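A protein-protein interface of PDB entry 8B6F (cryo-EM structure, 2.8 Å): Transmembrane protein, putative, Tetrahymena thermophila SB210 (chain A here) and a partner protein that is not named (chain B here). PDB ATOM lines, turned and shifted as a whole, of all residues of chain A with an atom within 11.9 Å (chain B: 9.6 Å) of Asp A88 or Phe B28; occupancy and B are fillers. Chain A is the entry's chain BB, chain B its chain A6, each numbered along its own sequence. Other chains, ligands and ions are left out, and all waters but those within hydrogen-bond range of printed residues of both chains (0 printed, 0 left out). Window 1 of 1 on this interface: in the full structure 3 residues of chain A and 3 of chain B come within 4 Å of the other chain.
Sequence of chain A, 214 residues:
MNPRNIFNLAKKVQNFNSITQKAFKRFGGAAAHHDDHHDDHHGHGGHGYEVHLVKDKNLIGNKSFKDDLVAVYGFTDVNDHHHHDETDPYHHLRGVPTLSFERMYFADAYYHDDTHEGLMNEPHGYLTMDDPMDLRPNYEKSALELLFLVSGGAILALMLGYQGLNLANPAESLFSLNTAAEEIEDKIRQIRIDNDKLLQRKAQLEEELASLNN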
ATOM      1  N   HIS A  84     -26.008  -4.109  -5.608  1.00  0.00           N
ATOM      2  CA  HIS A  84     -25.568  -5.054  -4.587  1.00  0.00           C
ATOM      3  C   HIS A  84     -26.500  -6.259  -4.599  1.00  0.00           C
ATOM      4  O   HIS A  84     -27.638  -6.178  -4.129  1.00  0.00           O
ATOM      5  CB  HIS A  84     -25.548  -4.387  -3.216  1.00  0.00           C
ATOM      6  CG  HIS A  84     -24.957  -5.243  -2.139  1.00  0.00           C
ATOM      7  ND1 HIS A  84     -23.665  -5.722  -2.195  1.00  0.00           N
ATOM      8  CD2 HIS A  84     -25.479  -5.706  -0.979  1.00  0.00           C
ATOM      9  CE1 HIS A  84     -23.417  -6.442  -1.115  1.00  0.00           C
ATOM     10  NE2 HIS A  84     -24.502  -6.448  -0.361  1.00  0.00           N
ATOM     11  N   ASP A  85     -26.016  -7.376  -5.136  1.00  0.00           N
ATOM     12  CA  ASP A  85     -26.788  -8.608  -5.225  1.00  0.00           C
ATOM     13  C   ASP A  85     -26.379  -9.531  -4.084  1.00  0.00           C
ATOM     14  O   ASP A  85     -25.209  -9.921  -3.985  1.00  0.00           O
ATOM     15  CB  ASP A  85     -26.568  -9.289  -6.575  1.00  0.00           C
ATOM     16  CG  ASP A  85     -27.498 -10.466  -6.793  1.00  0.00           C
ATOM     17  OD1 ASP A  85     -28.340 -10.731  -5.911  1.00  0.00           O
ATOM     18  OD2 ASP A  85     -27.388 -11.123  -7.849  1.00  0.00           O
ATOM     19  N   GLU A  86     -27.340  -9.877  -3.228  1.00  0.00           N
ATOM     20  CA  GLU A  86     -27.106 -10.747  -2.083  1.00  0.00           C
ATOM     21  C   GLU A  86     -27.795 -12.099  -2.246  1.00  0.00           C
ATOM     22  O   GLU A  86     -28.238 -12.699  -1.263  1.00  0.00           O
ATOM     23  CB  GLU A  86     -27.568 -10.067  -0.795  1.00  0.00           C
ATOM     24  CG  GLU A  86     -26.642  -8.966  -0.311  1.00  0.00           C
ATOM     25  CD  GLU A  86     -25.319  -9.503   0.204  1.00  0.00           C
ATOM     26  OE1 GLU A  86     -25.146 -10.739   0.225  1.00  0.00           O
ATOM     27  OE2 GLU A  86     -24.454  -8.691   0.593  1.00  0.00           O
ATOM     28  N   THR A  87     -27.897 -12.589  -3.479  1.00  0.00           N
ATOM     29  CA  THR A  87     -28.492 -13.898  -3.706  1.00  0.00           C
ATOM     30  C   THR A  87     -27.723 -14.957  -2.928  1.00  0.00           C
ATOM     31  O   THR A  87     -26.490 -14.960  -2.902  1.00  0.00           O
ATOM     32  CB  THR A  87     -28.502 -14.234  -5.198  1.00  0.00           C
ATOM     33  OG1 THR A  87     -29.135 -15.504  -5.402  1.00  0.00           O
ATOM     34  CG2 THR A  87     -27.085 -14.278  -5.758  1.00  0.00           C
ATOM     35  N   ASP A  88     -28.461 -15.859  -2.284  1.00  0.00           N
ATOM     36  CA  ASP A  88     -27.856 -16.840  -1.396  1.00  0.00           C
ATOM     37  C   ASP A  88     -27.594 -18.130  -2.157  1.00  0.00           C
ATOM     38  O   ASP A  88     -28.556 -18.819  -2.532  1.00  0.00           O
ATOM     39  CB  ASP A  88     -28.760 -17.112  -0.205  1.00  0.00           C
ATOM     40  CG  ASP A  88     -28.378 -18.379   0.535  1.00  0.00           C
ATOM     41  OD1 ASP A  88     -27.301 -18.403   1.162  1.00  0.00           O
ATOM     42  OD2 ASP A  88     -29.154 -19.355   0.486  1.00  0.00           O
ATOM     43  N   PRO A  89     -26.341 -18.503  -2.410  1.00  0.00           N
ATOM     44  CA  PRO A  89     -26.074 -19.860  -2.888  1.00  0.00           C
ATOM     45  C   PRO A  89     -26.350 -20.872  -1.791  1.00  0.00           C
ATOM     46  O   PRO A  89     -26.298 -20.562  -0.599  1.00  0.00           O
ATOM     47  CB  PRO A  89     -24.588 -19.825  -3.261  1.00  0.00           C
ATOM     48  CG  PRO A  89     -24.021 -18.734  -2.437  1.00  0.00           C
ATOM     49  CD  PRO A  89     -25.105 -17.709  -2.300  1.00  0.00           C
ATOM     50  N   TYR A  90     -26.656 -22.096  -2.206  1.00  0.00           N
ATOM     51  CA  TYR A  90     -27.026 -23.186  -1.313  1.00  0.00           C
ATOM     52  C   TYR A  90     -28.388 -22.967  -0.673  1.00  0.00           C
ATOM     53  O   TYR A  90     -28.723 -23.652   0.299  1.00  0.00           O
ATOM     54  CB  TYR A  90     -25.978 -23.394  -0.213  1.00  0.00           C
ATOM     55  CG  TYR A  90     -24.556 -23.322  -0.719  1.00  0.00           C
ATOM     56  CD1 TYR A  90     -24.038 -24.317  -1.535  1.00  0.00           C
ATOM     57  CD2 TYR A  90     -23.730 -22.263  -0.371  1.00  0.00           C
ATOM     58  CE1 TYR A  90     -22.742 -24.256  -1.999  1.00  0.00           C
ATOM     59  CE2 TYR A  90     -22.430 -22.193  -0.829  1.00  0.00           C
ATOM     60  CZ  TYR A  90     -21.942 -23.194  -1.640  1.00  0.00           C
ATOM     61  OH  TYR A  90     -20.648 -23.131  -2.099  1.00  0.00           O
ATOM     62  N   HIS A  91     -29.185 -22.031  -1.192  1.00  0.00           N
ATOM     63  CA  HIS A  91     -30.546 -21.857  -0.698  1.00  0.00           C
ATOM     64  C   HIS A  91     -31.333 -23.153  -0.812  1.00  0.00           C
ATOM     65  O   HIS A  91     -32.100 -23.509   0.090  1.00  0.00           O
ATOM     66  CB  HIS A  91     -31.243 -20.736  -1.465  1.00  0.00           C
ATOM     67  CG  HIS A  91     -32.689 -20.575  -1.113  1.00  0.00           C
ATOM     68  ND1 HIS A  91     -33.708 -20.969  -1.953  1.00  0.00           N
ATOM     69  CD2 HIS A  91     -33.287 -20.068  -0.009  1.00  0.00           C
ATOM     70  CE1 HIS A  91     -34.871 -20.709  -1.383  1.00  0.00           C
ATOM     71  NE2 HIS A  91     -34.643 -20.162  -0.203  1.00  0.00           N
ATOM     72  N   HIS A  92     -31.155 -23.874  -1.919  1.00  0.00           N
ATOM     73  CA  HIS A  92     -31.780 -25.182  -2.062  1.00  0.00           C
ATOM     74  C   HIS A  92     -31.306 -26.149  -0.987  1.00  0.00           C
ATOM     75  O   HIS A  92     -32.071 -27.019  -0.560  1.00  0.00           O
ATOM     76  CB  HIS A  92     -31.490 -25.746  -3.454  1.00  0.00           C
ATOM     77  CG  HIS A  92     -30.032 -25.844  -3.777  1.00  0.00           C
ATOM     78  ND1 HIS A  92     -29.350 -27.042  -3.786  1.00  0.00           N
ATOM     79  CD2 HIS A  92     -29.124 -24.894  -4.103  1.00  0.00           C
ATOM     80  CE1 HIS A  92     -28.086 -26.825  -4.102  1.00  0.00           C
ATOM     81  NE2 HIS A  92     -27.923 -25.530  -4.301  1.00  0.00           N
ATOM     82  N   LEU A  93     -30.055 -26.022  -0.542  1.00  0.00           N
ATOM     83  CA  LEU A  93     -29.535 -26.911   0.492  1.00  0.00           C
ATOM     84  C   LEU A  93     -30.050 -26.560   1.880  1.00  0.00           C
ATOM     85  O   LEU A  93     -30.122 -27.441   2.743  1.00  0.00           O
ATOM     86  CB  LEU A  93     -28.007 -26.878   0.493  1.00  0.00           C
ATOM     87  CG  LEU A  93     -27.322 -27.412  -0.765  1.00  0.00           C
ATOM     88  CD1 LEU A  93     -25.818 -27.326  -0.629  1.00  0.00           C
ATOM     89  CD2 LEU A  93     -27.746 -28.844  -1.053  1.00  0.00           C
ATOM     90  N   ARG A  94     -30.399 -25.299   2.123  1.00  0.00           N
ATOM     91  CA  ARG A  94     -30.864 -24.894   3.444  1.00  0.00           C
ATOM     92  C   ARG A  94     -32.032 -25.763   3.888  1.00  0.00           C
ATOM     93  O   ARG A  94     -33.042 -25.873   3.191  1.00  0.00           O
ATOM     94  CB  ARG A  94     -31.288 -23.422   3.432  1.00  0.00           C
ATOM     95  CG  ARG A  94     -30.220 -22.454   2.946  1.00  0.00           C
ATOM     96  CD  ARG A  94     -28.985 -22.461   3.824  1.00  0.00           C
ATOM     97  NE  ARG A  94     -27.948 -21.590   3.283  1.00  0.00           N
ATOM     98  CZ  ARG A  94     -26.737 -21.453   3.802  1.00  0.00           C
ATOM     99  NH1 ARG A  94     -26.371 -22.116   4.886  1.00  0.00           N
ATOM    100  NH2 ARG A  94     -25.870 -20.631   3.220  1.00  0.00           N
ATOM    101  N   GLY A  95     -31.889 -26.374   5.063  1.00  0.00           N
ATOM    102  CA  GLY A  95     -32.943 -27.198   5.624  1.00  0.00           C
ATOM    103  C   GLY A  95     -33.272 -28.429   4.805  1.00  0.00           C
ATOM    104  O   GLY A  95     -34.446 -28.720   4.558  1.00  0.00           O
ATOM    105  N   VAL A  96     -32.247 -29.161   4.377  1.00  0.00           N
ATOM    106  CA  VAL A  96     -32.433 -30.377   3.589  1.00  0.00           C
ATOM    107  C   VAL A  96     -31.702 -31.525   4.279  1.00  0.00           C
ATOM    108  O   VAL A  96     -30.601 -31.318   4.808  1.00  0.00           O
ATOM    109  CB  VAL A  96     -31.929 -30.178   2.150  1.00  0.00           C
ATOM    110  CG1 VAL A  96     -32.094 -31.437   1.338  1.00  0.00           C
ATOM    111  CG2 VAL A  96     -32.672 -29.041   1.487  1.00  0.00           C
ATOM    112  N   PHE A 106     -26.528 -32.614  -6.176  1.00  0.00           N
ATOM    113  CA  PHE A 106     -26.809 -31.287  -6.710  1.00  0.00           C
ATOM    114  C   PHE A 106     -26.511 -30.183  -5.703  1.00  0.00           C
ATOM    115  O   PHE A 106     -27.174 -29.142  -5.713  1.00  0.00           O
ATOM    116  CB  PHE A 106     -28.264 -31.207  -7.169  1.00  0.00           C
ATOM    117  CG  PHE A 106     -28.683 -32.341  -8.061  1.00  0.00           C
ATOM    118  CD1 PHE A 106     -27.787 -32.909  -8.954  1.00  0.00           C
ATOM    119  CD2 PHE A 106     -29.970 -32.846  -8.000  1.00  0.00           C
ATOM    120  CE1 PHE A 106     -28.171 -33.955  -9.772  1.00  0.00           C
ATOM    121  CE2 PHE A 106     -30.358 -33.892  -8.813  1.00  0.00           C
ATOM    122  CZ  PHE A 106     -29.458 -34.447  -9.701  1.00  0.00           C
ATOM    123  N   ALA A 107     -25.527 -30.388  -4.835  1.00  0.00           N
ATOM    124  CA  ALA A 107     -25.166 -29.397  -3.822  1.00  0.00           C
ATOM    125  C   ALA A 107     -24.198 -28.357  -4.373  1.00  0.00           C
ATOM    126  O   ALA A 107     -23.127 -28.117  -3.820  1.00  0.00           O
ATOM    127  CB  ALA A 107     -24.576 -30.101  -2.607  1.00  0.00           C
ATOM    128  N   ASP A 108     -24.583 -27.719  -5.475  1.00  0.00           N
ATOM    129  CA  ASP A 108     -23.758 -26.719  -6.128  1.00  0.00           C
ATOM    130  C   ASP A 108     -24.156 -25.323  -5.662  1.00  0.00           C
ATOM    131  O   ASP A 108     -25.095 -25.137  -4.886  1.00  0.00           O
ATOM    132  CB  ASP A 108     -23.869 -26.853  -7.647  1.00  0.00           C
ATOM    133  CG  ASP A 108     -23.144 -28.072  -8.172  1.00  0.00           C
ATOM    134  OD1 ASP A 108     -21.939 -28.218  -7.881  1.00  0.00           O
ATOM    135  OD2 ASP A 108     -23.779 -28.895  -8.859  1.00  0.00           O
ATOM    136  N   ALA A 109     -23.423 -24.323  -6.152  1.00  0.00           N
ATOM    137  CA  ALA A 109     -23.593 -22.965  -5.649  1.00  0.00           C
ATOM    138  C   ALA A 109     -24.979 -22.419  -5.972  1.00  0.00           C
ATOM    139  O   ALA A 109     -25.681 -21.916  -5.087  1.00  0.00           O
ATOM    140  CB  ALA A 109     -22.509 -22.057  -6.229  1.00  0.00           C
ATOM    141  N   TYR A 110     -25.393 -22.514  -7.233  1.00  0.00           N
ATOM    142  CA  TYR A 110     -26.616 -21.874  -7.713  1.00  0.00           C
ATOM    143  C   TYR A 110     -27.495 -22.872  -8.454  1.00  0.00           C
ATOM    144  O   TYR A 110     -28.015 -22.599  -9.537  1.00  0.00           O
ATOM    145  CB  TYR A 110     -26.276 -20.686  -8.607  1.00  0.00           C
ATOM    146  CG  TYR A 110     -25.451 -19.624  -7.918  1.00  0.00           C
ATOM    147  CD1 TYR A 110     -26.060 -18.617  -7.179  1.00  0.00           C
ATOM    148  CD2 TYR A 110     -24.066 -19.627  -8.004  1.00  0.00           C
ATOM    149  CE1 TYR A 110     -25.312 -17.644  -6.547  1.00  0.00           C
ATOM    150  CE2 TYR A 110     -23.309 -18.659  -7.375  1.00  0.00           C
ATOM    151  CZ  TYR A 110     -23.939 -17.671  -6.649  1.00  0.00           C
ATOM    152  OH  TYR A 110     -23.189 -16.704  -6.021  1.00  0.00           O
ATOM    153  N   TYR A 111     -27.676 -24.052  -7.870  1.00  0.00           N
ATOM    154  CA  TYR A 111     -28.566 -25.045  -8.454  1.00  0.00           C
ATOM    155  C   TYR A 111     -30.015 -24.587  -8.355  1.00  0.00           C
ATOM    156  O   TYR A 111     -30.442 -24.040  -7.335  1.00  0.00           O
ATOM    157  CB  TYR A 111     -28.388 -26.388  -7.752  1.00  0.00           C
ATOM    158  CG  TYR A 111     -29.400 -27.437  -8.150  1.00  0.00           C
ATOM    159  CD1 TYR A 111     -29.350 -28.039  -9.398  1.00  0.00           C
ATOM    160  CD2 TYR A 111     -30.396 -27.835  -7.269  1.00  0.00           C
ATOM    161  CE1 TYR A 111     -30.269 -29.002  -9.764  1.00  0.00           C
ATOM    162  CE2 TYR A 111     -31.321 -28.797  -7.625  1.00  0.00           C
ATOM    163  CZ  TYR A 111     -31.252 -29.376  -8.874  1.00  0.00           C
ATOM    164  OH  TYR A 111     -32.168 -30.336  -9.234  1.00  0.00           O
ATOM    165  N   HIS A 112     -30.775 -24.815  -9.424  1.00  0.00           N
ATOM    166  CA  HIS A 112     -32.185 -24.457  -9.489  1.00  0.00           C
ATOM    167  C   HIS A 112     -33.035 -25.714  -9.369  1.00  0.00           C
ATOM    168  O   HIS A 112     -32.799 -26.698 -10.078  1.00  0.00           O
ATOM    169  CB  HIS A 112     -32.508 -23.729 -10.794  1.00  0.00           C
ATOM    170  CG  HIS A 112     -31.854 -22.389 -10.912  1.00  0.00           C
ATOM    171  ND1 HIS A 112     -32.188 -21.324 -10.103  1.00  0.00           N
ATOM    172  CD2 HIS A 112     -30.888 -21.938 -11.745  1.00  0.00           C
ATOM    173  CE1 HIS A 112     -31.454 -20.276 -10.431  1.00  0.00           C
ATOM    174  NE2 HIS A 112     -30.657 -20.622 -11.426  1.00  0.00           N
ATOM    175  N   ASP A 113     -34.026 -25.675  -8.483  1.00  0.00           N
ATOM    176  CA  ASP A 113     -34.887 -26.826  -8.268  1.00  0.00           C
ATOM    177  C   ASP A 113     -35.742 -27.098  -9.502  1.00  0.00           C
ATOM    178  O   ASP A 113     -36.000 -26.215 -10.325  1.00  0.00           O
ATOM    179  CB  ASP A 113     -35.789 -26.602  -7.054  1.00  0.00           C
ATOM    180  CG  ASP A 113     -35.002 -26.338  -5.786  1.00  0.00           C
ATOM    181  OD1 ASP A 113     -33.856 -26.824  -5.686  1.00  0.00           O
ATOM    182  OD2 ASP A 113     -35.526 -25.647  -4.887  1.00  0.00           O
ATOM    183  N   GLY B  22     -20.168  -9.392   1.582  1.00  0.00           N
ATOM    184  CA  GLY B  22     -20.271 -10.500   0.593  1.00  0.00           C
ATOM    185  C   GLY B  22     -20.496 -11.851   1.241  1.00  0.00           C
ATOM    186  O   GLY B  22     -21.081 -12.746   0.636  1.00  0.00           O
ATOM    187  N   ASP B  23     -20.031 -11.999   2.479  1.00  0.00           N
ATOM    188  CA  ASP B  23     -20.176 -13.244   3.218  1.00  0.00           C
ATOM    189  C   ASP B  23     -21.513 -13.253   3.948  1.00  0.00           C
ATOM    190  O   ASP B  23     -21.882 -12.264   4.589  1.00  0.00           O
ATOM    191  CB  ASP B  23     -19.024 -13.410   4.210  1.00  0.00           C
ATOM    192  CG  ASP B  23     -18.944 -14.810   4.780  1.00  0.00           C
ATOM    193  OD1 ASP B  23     -19.734 -15.674   4.348  1.00  0.00           O
ATOM    194  OD2 ASP B  23     -18.091 -15.045   5.661  1.00  0.00           O
ATOM    195  N   ILE B  24     -22.232 -14.369   3.850  1.00  0.00           N
ATOM    196  CA  ILE B  24     -23.563 -14.496   4.428  1.00  0.00           C
ATOM    197  C   ILE B  24     -23.638 -15.660   5.416  1.00  0.00           C
ATOM    198  O   ILE B  24     -24.721 -16.137   5.729  1.00  0.00           O
ATOM    199  CB  ILE B  24     -24.631 -14.637   3.326  1.00  0.00           C
ATOM    200  CG1 ILE B  24     -24.374 -15.898   2.496  1.00  0.00           C
ATOM    201  CG2 ILE B  24     -24.629 -13.397   2.439  1.00  0.00           C
ATOM    202  CD1 ILE B  24     -25.402 -16.151   1.413  1.00  0.00           C
ATOM    203  N   ARG B  25     -22.490 -16.123   5.912  1.00  0.00           N
ATOM    204  CA  ARG B  25     -22.493 -17.226   6.867  1.00  0.00           C
ATOM    205  C   ARG B  25     -23.173 -16.840   8.174  1.00  0.00           C
ATOM    206  O   ARG B  25     -23.724 -17.704   8.863  1.00  0.00           O
ATOM    207  CB  ARG B  25     -21.062 -17.689   7.136  1.00  0.00           C
ATOM    208  CG  ARG B  25     -20.439 -18.459   5.985  1.00  0.00           C
ATOM    209  CD  ARG B  25     -18.928 -18.322   5.987  1.00  0.00           C
ATOM    210  NE  ARG B  25     -18.346 -18.657   7.279  1.00  0.00           N
ATOM    211  CZ  ARG B  25     -17.084 -18.429   7.614  1.00  0.00           C
ATOM    212  NH1 ARG B  25     -16.240 -17.852   6.775  1.00  0.00           N
ATOM    213  NH2 ARG B  25     -16.660 -18.782   8.823  1.00  0.00           N
ATOM    214  N   HIS B  26     -23.149 -15.556   8.530  1.00  0.00           N
ATOM    215  CA  HIS B  26     -23.734 -15.122   9.792  1.00  0.00           C
ATOM    216  C   HIS B  26     -25.255 -15.201   9.789  1.00  0.00           C
ATOM    217  O   HIS B  26     -25.863 -15.198  10.864  1.00  0.00           O
ATOM    218  CB  HIS B  26     -23.295 -13.692  10.109  1.00  0.00           C
ATOM    219  CG  HIS B  26     -23.693 -12.697   9.065  1.00  0.00           C
ATOM    220  ND1 HIS B  26     -22.897 -12.397   7.980  1.00  0.00           N
ATOM    221  CD2 HIS B  26     -24.804 -11.934   8.938  1.00  0.00           C
ATOM    222  CE1 HIS B  26     -23.499 -11.492   7.232  1.00  0.00           C
ATOM    223  NE2 HIS B  26     -24.658 -11.194   7.790  1.00  0.00           N
ATOM    224  N   LYS B  27     -25.883 -15.267   8.615  1.00  0.00           N
ATOM    225  CA  LYS B  27     -27.339 -15.301   8.539  1.00  0.00           C
ATOM    226  C   LYS B  27     -27.929 -16.632   8.984  1.00  0.00           C
ATOM    227  O   LYS B  27     -29.150 -16.718   9.150  1.00  0.00           O
ATOM    228  CB  LYS B  27     -27.796 -14.996   7.113  1.00  0.00           C
ATOM    229  CG  LYS B  27     -27.507 -13.575   6.664  1.00  0.00           C
ATOM    230  CD  LYS B  27     -27.986 -13.337   5.242  1.00  0.00           C
ATOM    231  CE  LYS B  27     -27.820 -11.880   4.843  1.00  0.00           C
ATOM    232  NZ  LYS B  27     -26.421 -11.403   5.016  1.00  0.00           N
ATOM    233  N   PHE B  28     -27.109 -17.660   9.177  1.00  0.00           N
ATOM    234  CA  PHE B  28     -27.589 -18.987   9.533  1.00  0.00           C
ATOM    235  C   PHE B  28     -26.899 -19.454  10.804  1.00  0.00           C
ATOM    236  O   PHE B  28     -25.691 -19.265  10.973  1.00  0.00           O
ATOM    237  CB  PHE B  28     -27.341 -19.978   8.393  1.00  0.00           C
ATOM    238  CG  PHE B  28     -27.865 -19.510   7.069  1.00  0.00           C
ATOM    239  CD1 PHE B  28     -27.081 -18.727   6.238  1.00  0.00           C
ATOM    240  CD2 PHE B  28     -29.144 -19.842   6.658  1.00  0.00           C
ATOM    241  CE1 PHE B  28     -27.560 -18.288   5.020  1.00  0.00           C
ATOM    242  CE2 PHE B  28     -29.630 -19.406   5.440  1.00  0.00           C
ATOM    243  CZ  PHE B  28     -28.836 -18.628   4.621  1.00  0.00           C
ATOM    244  N   SER B  29     -27.678 -20.062  11.702  1.00  0.00           N
ATOM    245  CA  SER B  29     -27.148 -20.481  12.992  1.00  0.00           C
ATOM    246  C   SER B  29     -26.298 -21.741  12.888  1.00  0.00           C
ATOM    247  O   SER B  29     -25.400 -21.942  13.713  1.00  0.00           O
ATOM    248  CB  SER B  29     -28.294 -20.708  13.980  1.00  0.00           C
ATOM    249  OG  SER B  29     -29.198 -21.685  13.495  1.00  0.00           O
ATOM    250  N   ASN B  30     -26.557 -22.591  11.898  1.00  0.00           N
ATOM    251  CA  ASN B  30     -25.851 -23.855  11.749  1.00  0.00           C
ATOM    252  C   ASN B  30     -24.755 -23.795  10.693  1.00  0.00           C
ATOM    253  O   ASN B  30     -24.265 -24.843  10.264  1.00  0.00           O
ATOM    254  CB  ASN B  30     -26.836 -24.973  11.406  1.00  0.00           C
ATOM    255  CG  ASN B  30     -27.419 -24.829  10.017  1.00  0.00           C
ATOM    256  OD1 ASN B  30     -27.629 -23.718   9.531  1.00  0.00           O
ATOM    257  ND2 ASN B  30     -27.680 -25.956   9.366  1.00  0.00           N
ATOM    258  N   GLU B  31     -24.366 -22.600  10.261  1.00  0.00           N
ATOM    259  CA  GLU B  31     -23.339 -22.471   9.242  1.00  0.00           C
ATOM    260  C   GLU B  31     -21.952 -22.627   9.858  1.00  0.00           C
ATOM    261  O   GLU B  31     -21.740 -22.399  11.051  1.00  0.00           O
ATOM    262  CB  GLU B  31     -23.449 -21.121   8.535  1.00  0.00           C
ATOM    263  CG  GLU B  31     -22.673 -21.038   7.229  1.00  0.00           C
ATOM    264  CD  GLU B  31     -23.162 -22.030   6.195  1.00  0.00           C
ATOM    265  OE1 GLU B  31     -24.315 -22.493   6.310  1.00  0.00           O
ATOM    266  OE2 GLU B  31     -22.394 -22.351   5.267  1.00  0.00           O
ATOM    267  N   ILE B  32     -20.997 -23.026   9.016  1.00  0.00           N
ATOM    268  CA  ILE B  32     -19.640 -23.241   9.489  1.00  0.00           C
ATOM    269  C   ILE B  32     -19.057 -21.929  10.011  1.00  0.00           C
ATOM    270  O   ILE B  32     -19.495 -20.829   9.651  1.00  0.00           O
ATOM    271  CB  ILE B  32     -18.768 -23.840   8.373  1.00  0.00           C
ATOM    272  CG1 ILE B  32     -17.452 -24.362   8.947  1.00  0.00           C
ATOM    273  CG2 ILE B  32     -18.502 -22.807   7.282  1.00  0.00           C
ATOM    274  CD1 ILE B  32     -16.731 -25.306   8.022  1.00  0.00           C
ATOM    275  N   THR B  33     -18.054 -22.054  10.877  1.00  0.00           N
ATOM    276  CA  THR B  33     -17.444 -20.917  11.547  1.00  0.00           C
ATOM    277  C   THR B  33     -15.928 -21.027  11.471  1.00  0.00           C
ATOM    278  O   THR B  33     -15.374 -22.090  11.185  1.00  0.00           O
ATOM    279  CB  THR B  33     -17.884 -20.826  13.016  1.00  0.00           C
ATOM    280  OG1 THR B  33     -17.563 -22.048  13.694  1.00  0.00           O
ATOM    281  CG2 THR B  33     -19.379 -20.576  13.113  1.00  0.00           C
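The guanidinium group (NH1) of Arg A94 lies within salt-bridge range of the side-chain carboxylate (OE1) of Glu B31 (2.5 Å).
NE2 of His A84 lies within hydrogen-bond range of OE2 of Glu A86. OD2 of Asp A88 lies close to N of His A91, 3.2 Å away. OD1 of Asp A88 lies within salt-bridge range of NH2 of Arg A94.
Ile B24 touches Glu A86 (CG2 to OE1, 3.5 Å). Asp A88 touches Ile B24 (OD1 to CD1, 3.0 Å). OD1 of Asp A88 touches CZ of Phe B28, at 3.8 Å. NE of Arg A94 touches CZ of Phe B28 (3.4 Å).
Asp A88 touches just these residues of chain B: Ile B24 (3.0 Å) and Phe B28 (3.8 Å). Phe B28 touches two residues of chain A. No residue of chain B comes within 4 Å of Pro A89. No residue of chain A comes within 4 Å of His B26. No residue of chain A comes within 4 Å of Lys B27. No residue of chain A comes within 4 Å of Asn B30. Of chain A, only Arg A94 comes within 4 Å of Glu B31. Printed residues of chain B within 4 Å of Glu A86: Ile B24. Of the printed residues of chain B, Arg A94 touches Phe B28 and Glu B31. Val A96 touches none of the printed residues of chain B. The nearest residue of chain B that does not touch Asp A88 is Lys B27 (6.5 Å). The nearest residue of chain A that does not touch Phe B28 is Pro A89 (6.1 Å).
Printed residues of chain B that touch a printed residue of chain A: Ile B24, Phe B28 and Glu B31. Hydrophobic or aromatic side chains of chain B that line the printed part of chain A: Ile B24 and Phe B28. Along chain B the printed residues that touch a printed residue of chain A span positions 24 to 31. Among the printed residues, 5 pairs touch across the chains. Among the printed residues, Asp or Glu carboxylates within 4 Å of a Lys or Arg side-chain nitrogen of the other chain: Arg A94 with Glu B31 (2.5 Å).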
